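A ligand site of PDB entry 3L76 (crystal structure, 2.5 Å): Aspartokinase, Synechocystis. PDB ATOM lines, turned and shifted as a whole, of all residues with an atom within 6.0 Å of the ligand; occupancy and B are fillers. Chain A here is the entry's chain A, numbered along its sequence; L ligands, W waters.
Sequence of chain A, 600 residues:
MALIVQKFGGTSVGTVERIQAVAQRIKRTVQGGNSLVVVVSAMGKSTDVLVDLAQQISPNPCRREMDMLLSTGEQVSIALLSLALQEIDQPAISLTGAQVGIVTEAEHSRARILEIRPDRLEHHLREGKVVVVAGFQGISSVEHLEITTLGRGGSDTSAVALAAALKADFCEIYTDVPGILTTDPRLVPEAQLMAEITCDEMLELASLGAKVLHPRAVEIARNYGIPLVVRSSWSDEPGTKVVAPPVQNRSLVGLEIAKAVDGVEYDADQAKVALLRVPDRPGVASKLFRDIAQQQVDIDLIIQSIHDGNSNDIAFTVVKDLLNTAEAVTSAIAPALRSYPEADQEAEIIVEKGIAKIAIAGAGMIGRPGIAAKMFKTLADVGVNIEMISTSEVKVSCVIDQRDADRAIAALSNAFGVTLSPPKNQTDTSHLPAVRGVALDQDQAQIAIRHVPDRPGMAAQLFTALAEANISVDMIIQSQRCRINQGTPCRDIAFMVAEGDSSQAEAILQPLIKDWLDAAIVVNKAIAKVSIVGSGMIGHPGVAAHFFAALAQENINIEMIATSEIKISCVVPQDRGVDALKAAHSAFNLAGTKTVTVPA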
ATOM      1  N   VAL A 278     -30.556  -6.917  24.118  1.00  0.00           N
ATOM      2  CA  VAL A 278     -30.808  -5.499  23.954  1.00  0.00           C
ATOM      3  C   VAL A 278     -30.926  -5.259  22.437  1.00  0.00           C
ATOM      4  O   VAL A 278     -30.487  -6.085  21.644  1.00  0.00           O
ATOM      5  CB  VAL A 278     -29.653  -4.692  24.621  1.00  0.00           C
ATOM      6  CG1 VAL A 278     -28.549  -4.398  23.625  1.00  0.00           C
ATOM      7  CG2 VAL A 278     -30.153  -3.407  25.229  1.00  0.00           C
ATOM      8  N   PRO A 279     -31.553  -4.131  22.026  1.00  0.00           N
ATOM      9  CA  PRO A 279     -31.703  -3.892  20.577  1.00  0.00           C
ATOM     10  C   PRO A 279     -30.361  -3.642  19.882  1.00  0.00           C
ATOM     11  O   PRO A 279     -29.509  -2.920  20.407  1.00  0.00           O
ATOM     12  CB  PRO A 279     -32.574  -2.625  20.515  1.00  0.00           C
ATOM     13  CG  PRO A 279     -33.269  -2.564  21.838  1.00  0.00           C
ATOM     14  CD  PRO A 279     -32.302  -3.167  22.836  1.00  0.00           C
ATOM     15  N   ASP A 280     -30.183  -4.210  18.696  1.00  0.00           N
ATOM     16  CA  ASP A 280     -28.941  -4.025  17.947  1.00  0.00           C
ATOM     17  C   ASP A 280     -29.000  -2.827  17.008  1.00  0.00           C
ATOM     18  O   ASP A 280     -29.146  -2.984  15.808  1.00  0.00           O
ATOM     19  CB  ASP A 280     -28.588  -5.279  17.143  1.00  0.00           C
ATOM     20  CG  ASP A 280     -27.287  -5.134  16.369  1.00  0.00           C
ATOM     21  OD1 ASP A 280     -26.445  -4.269  16.742  1.00  0.00           O
ATOM     22  OD2 ASP A 280     -27.087  -5.874  15.385  1.00  0.00           O
ATOM     23  N   ARG A 281     -28.879  -1.643  17.582  1.00  0.00           N
ATOM     24  CA  ARG A 281     -28.924  -0.409  16.804  1.00  0.00           C
ATOM     25  C   ARG A 281     -27.999   0.624  17.440  1.00  0.00           C
ATOM     26  O   ARG A 281     -27.657   0.506  18.608  1.00  0.00           O
ATOM     27  CB  ARG A 281     -30.354   0.132  16.773  1.00  0.00           C
ATOM     28  CG  ARG A 281     -30.934   0.422  18.144  1.00  0.00           C
ATOM     29  CD  ARG A 281     -32.240   1.198  18.070  1.00  0.00           C
ATOM     30  NE  ARG A 281     -32.764   1.464  19.403  1.00  0.00           N
ATOM     31  CZ  ARG A 281     -33.860   0.904  19.915  1.00  0.00           C
ATOM     32  NH1 ARG A 281     -34.593   0.066  19.183  1.00  0.00           N
ATOM     33  NH2 ARG A 281     -34.236   1.200  21.150  1.00  0.00           N
ATOM     34  N   PRO A 282     -27.588   1.637  16.664  1.00  0.00           N
ATOM     35  CA  PRO A 282     -26.746   2.693  17.224  1.00  0.00           C
ATOM     36  C   PRO A 282     -27.375   3.342  18.466  1.00  0.00           C
ATOM     37  O   PRO A 282     -28.587   3.550  18.527  1.00  0.00           O
ATOM     38  CB  PRO A 282     -26.677   3.712  16.076  1.00  0.00           C
ATOM     39  CG  PRO A 282     -26.882   2.916  14.859  1.00  0.00           C
ATOM     40  CD  PRO A 282     -27.867   1.856  15.238  1.00  0.00           C
ATOM     41  N   GLY A 283     -26.539   3.640  19.465  1.00  0.00           N
ATOM     42  CA  GLY A 283     -26.977   4.356  20.634  1.00  0.00           C
ATOM     43  C   GLY A 283     -27.122   3.528  21.894  1.00  0.00           C
ATOM     44  O   GLY A 283     -27.064   4.056  22.997  1.00  0.00           O
ATOM     45  N   VAL A 284     -27.308   2.225  21.727  1.00  0.00           N
ATOM     46  CA  VAL A 284     -27.529   1.353  22.865  1.00  0.00           C
ATOM     47  C   VAL A 284     -26.325   1.311  23.807  1.00  0.00           C
ATOM     48  O   VAL A 284     -26.433   1.648  24.990  1.00  0.00           O
ATOM     49  CB  VAL A 284     -27.909  -0.066  22.427  1.00  0.00           C
ATOM     50  CG1 VAL A 284     -28.209  -0.913  23.642  1.00  0.00           C
ATOM     51  CG2 VAL A 284     -29.102  -0.029  21.505  1.00  0.00           C
ATOM     52  N   ALA A 285     -25.159   0.909  23.288  1.00  0.00           N
ATOM     53  CA  ALA A 285     -23.988   0.809  24.170  1.00  0.00           C
ATOM     54  C   ALA A 285     -23.667   2.171  24.731  1.00  0.00           C
ATOM     55  O   ALA A 285     -23.354   2.297  25.910  1.00  0.00           O
ATOM     56  CB  ALA A 285     -22.784   0.226  23.426  1.00  0.00           C
ATOM     57  N   SER A 286     -23.756   3.198  23.880  1.00  0.00           N
ATOM     58  CA  SER A 286     -23.557   4.570  24.320  1.00  0.00           C
ATOM     59  C   SER A 286     -24.328   4.883  25.609  1.00  0.00           C
ATOM     60  O   SER A 286     -23.743   5.317  26.588  1.00  0.00           O
ATOM     61  CB  SER A 286     -23.967   5.544  23.222  1.00  0.00           C
ATOM     62  OG  SER A 286     -23.670   6.865  23.604  1.00  0.00           O
ATOM     63  N   GLN A 304     -18.589  -7.742  23.659  1.00  0.00           N
ATOM     64  CA  GLN A 304     -19.794  -7.896  22.867  1.00  0.00           C
ATOM     65  C   GLN A 304     -19.486  -8.672  21.588  1.00  0.00           C
ATOM     66  O   GLN A 304     -18.839  -8.163  20.677  1.00  0.00           O
ATOM     67  CB  GLN A 304     -20.385  -6.540  22.528  1.00  0.00           C
ATOM     68  CG  GLN A 304     -21.665  -6.635  21.682  1.00  0.00           C
ATOM     69  CD  GLN A 304     -22.146  -5.284  21.230  1.00  0.00           C
ATOM     70  OE1 GLN A 304     -22.446  -4.385  22.039  1.00  0.00           O
ATOM     71  NE2 GLN A 304     -22.211  -5.112  19.916  1.00  0.00           N
ATOM     72  N   ASN A 312     -28.441  -7.939  20.551  1.00  0.00           N
ATOM     73  CA  ASN A 312     -27.159  -8.434  21.054  1.00  0.00           C
ATOM     74  C   ASN A 312     -27.107  -8.430  22.579  1.00  0.00           C
ATOM     75  O   ASN A 312     -27.995  -7.877  23.213  1.00  0.00           O
ATOM     76  CB  ASN A 312     -26.005  -7.598  20.491  1.00  0.00           C
ATOM     77  CG  ASN A 312     -24.730  -8.391  20.325  1.00  0.00           C
ATOM     78  OD1 ASN A 312     -24.516  -9.406  20.977  1.00  0.00           O
ATOM     79  ND2 ASN A 312     -23.854  -7.922  19.443  1.00  0.00           N
ATOM     80  N   ASP A 313     -26.063  -9.034  23.148  1.00  0.00           N
ATOM     81  CA  ASP A 313     -25.803  -8.895  24.583  1.00  0.00           C
ATOM     82  C   ASP A 313     -24.630  -7.921  24.786  1.00  0.00           C
ATOM     83  O   ASP A 313     -23.806  -7.703  23.896  1.00  0.00           O
ATOM     84  CB  ASP A 313     -25.488 -10.231  25.214  1.00  0.00           C
ATOM     85  CG  ASP A 313     -26.518 -11.293  24.902  1.00  0.00           C
ATOM     86  OD1 ASP A 313     -27.737 -11.006  24.837  1.00  0.00           O
ATOM     87  OD2 ASP A 313     -26.085 -12.452  24.718  1.00  0.00           O
ATOM     88  N   ILE A 314     -24.574  -7.310  25.963  1.00  0.00           N
ATOM     89  CA  ILE A 314     -23.417  -6.523  26.347  1.00  0.00           C
ATOM     90  C   ILE A 314     -22.934  -6.967  27.736  1.00  0.00           C
ATOM     91  O   ILE A 314     -23.700  -6.977  28.702  1.00  0.00           O
ATOM     92  CB  ILE A 314     -23.707  -5.037  26.342  1.00  0.00           C
ATOM     93  CG1 ILE A 314     -24.160  -4.605  24.951  1.00  0.00           C
ATOM     94  CG2 ILE A 314     -22.468  -4.268  26.778  1.00  0.00           C
ATOM     95  CD1 ILE A 314     -24.474  -3.124  24.819  1.00  0.00           C
ATOM     96  N   ILE A 556     -23.410   5.360  13.818  1.00  0.00           N
ATOM     97  CA  ILE A 556     -22.588   4.224  13.431  1.00  0.00           C
ATOM     98  C   ILE A 556     -22.889   3.058  14.374  1.00  0.00           C
ATOM     99  O   ILE A 556     -22.790   3.169  15.590  1.00  0.00           O
ATOM    100  CB  ILE A 556     -21.077   4.587  13.466  1.00  0.00           C
ATOM    101  CG1 ILE A 556     -20.730   5.512  12.310  1.00  0.00           C
ATOM    102  CG2 ILE A 556     -20.197   3.367  13.403  1.00  0.00           C
ATOM    103  CD1 ILE A 556     -19.319   6.059  12.355  1.00  0.00           C
ATOM    104  N   ASN A 557     -23.291   1.933  13.797  1.00  0.00           N
ATOM    105  CA  ASN A 557     -23.646   0.800  14.632  1.00  0.00           C
ATOM    106  C   ASN A 557     -22.424   0.021  15.081  1.00  0.00           C
ATOM    107  O   ASN A 557     -21.492  -0.189  14.303  1.00  0.00           O
ATOM    108  CB  ASN A 557     -24.625  -0.123  13.903  1.00  0.00           C
ATOM    109  CG  ASN A 557     -25.134  -1.237  14.789  1.00  0.00           C
ATOM    110  OD1 ASN A 557     -25.653  -0.988  15.884  1.00  0.00           O
ATOM    111  ND2 ASN A 557     -24.988  -2.481  14.322  1.00  0.00           N
ATOM    112  N   ILE A 558     -22.437  -0.420  16.324  1.00  0.00           N
ATOM    113  CA  ILE A 558     -21.317  -1.183  16.854  1.00  0.00           C
ATOM    114  C   ILE A 558     -21.625  -2.663  16.821  1.00  0.00           C
ATOM    115  O   ILE A 558     -22.501  -3.148  17.540  1.00  0.00           O
ATOM    116  CB  ILE A 558     -20.977  -0.744  18.291  1.00  0.00           C
ATOM    117  CG1 ILE A 558     -20.694   0.761  18.333  1.00  0.00           C
ATOM    118  CG2 ILE A 558     -19.788  -1.552  18.816  1.00  0.00           C
ATOM    119  CD1 ILE A 558     -20.531   1.307  19.727  1.00  0.00           C
ATOM    120  N   GLU A 559     -20.912  -3.399  15.970  1.00  0.00           N
ATOM    121  CA  GLU A 559     -21.190  -4.807  15.756  1.00  0.00           C
ATOM    122  C   GLU A 559     -20.602  -5.692  16.855  1.00  0.00           C
ATOM    123  O   GLU A 559     -21.241  -6.618  17.336  1.00  0.00           O
ATOM    124  CB  GLU A 559     -20.690  -5.272  14.384  1.00  0.00           C
ATOM    125  CG  GLU A 559     -21.186  -4.436  13.196  1.00  0.00           C
ATOM    126  CD  GLU A 559     -20.949  -5.122  11.863  1.00  0.00           C
ATOM    127  OE1 GLU A 559     -20.875  -6.362  11.833  1.00  0.00           O
ATOM    128  OE2 GLU A 559     -20.856  -4.416  10.823  1.00  0.00           O
ATOM    129  N   ILE A 561     -17.588  -5.577  20.344  1.00  0.00           N
ATOM    130  CA  ILE A 561     -16.668  -4.825  21.192  1.00  0.00           C
ATOM    131  C   ILE A 561     -15.742  -5.806  21.886  1.00  0.00           C
ATOM    132  O   ILE A 561     -16.161  -6.879  22.311  1.00  0.00           O
ATOM    133  CB  ILE A 561     -17.397  -4.028  22.287  1.00  0.00           C
ATOM    134  CG1 ILE A 561     -18.474  -3.132  21.682  1.00  0.00           C
ATOM    135  CG2 ILE A 561     -16.423  -3.223  23.111  1.00  0.00           C
ATOM    136  CD1 ILE A 561     -19.476  -2.650  22.704  1.00  0.00           C
HETATM  137  N1  LIG L   1     -25.264  -2.060  18.220  1.00  0.00           N
HETATM  138  C1  LIG L   1     -25.433  -1.397  19.518  1.00  0.00           C
HETATM  139  C2  LIG L   1     -24.829   0.005  19.527  1.00  0.00           C
HETATM  140  O1  LIG L   1     -24.208   0.429  18.534  1.00  0.00           O
HETATM  141  C3  LIG L   1     -24.866  -2.230  20.687  1.00  0.00           C
HETATM  142  O2  LIG L   1     -23.448  -2.415  20.509  1.00  0.00           O
HETATM  143  C4  LIG L   1     -25.538  -3.600  20.711  1.00  0.00           C
HETATM  144  O3  LIG L   1     -24.970   0.734  20.515  1.00  0.00           O
HETATM  145  O   HOH W   1     -23.700   2.837  18.445  1.00  0.00           O
HETATM  146  O   HOH W   2     -23.757   3.019  21.078  1.00  0.00           O
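N of Ala 285 is in hydrogen-bond range of O3 of the ligand.
The backbone NH (N) of Ile 558 lies within hydrogen-bond range of an oxygen (O1) of the ligand (3.0 Å).
N of Gly 283 sits at hydrogen-bond distance from O3 of the ligand.
O of Ile 558 lies within hydrogen-bond range of N1 of the ligand, at 3.0 Å.
An oxygen (O2) of the ligand sits at hydrogen-bond distance from the side-chain amide oxygen (OE1) of Gln 304 (2.7 Å).
The side-chain amide oxygen of Asn 557 sits at hydrogen-bond distance from a nitrogen (N1) of the ligand, 2.6 Å away.
The side-chain carboxylate (OD1) of Asp 280 is in salt-bridge range of a nitrogen (N1) of the ligand.
An oxygen (O3) of the ligand lies within hydrogen-bond range of the backbone NH of Val 284 (3.0 Å).
NE2 of Gln 304 is in hydrogen-bond range of O of Glu 559 (3.1 Å).
The backbone NH of Ile 561 sits at hydrogen-bond distance from the backbone carbonyl oxygen of Gln 304 (2.9 Å).
The side-chain amide nitrogen (ND2) of Asn 312 sits close to the side-chain amide nitrogen (NE2) of Gln 304, at 3.3 Å.
The side-chain amide nitrogen of Asn 557 lies within hydrogen-bond range of the side-chain carboxylate of Asp 280, 3.3 Å away.
NE2 of Gln 304 sits at hydrogen-bond distance from O of Ile 558.
O3 of the ligand lies close to O of Arg 281 (3.3 Å).
Residues that only touch the ligand: Pro 282 (3.6 Å).
Hydrophobic or aromatic side chains within 4 Å of the ligand: Val 284, Ala 285 and Ile 558.
Nine residues have an atom within 4 Å of the ligand: Asp 280, Arg 281, Pro 282, Gly 283, Val 284, Ala 285, Gln 304, Asn 557 and Ile 558.
Water W1 lies within hydrogen-bond range of an oxygen (O1) of the ligand (2.5 Å), the backbone carbonyl oxygen of Ile 556 (3.0 Å) and the backbone NH of Gly 283 (3.1 Å).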
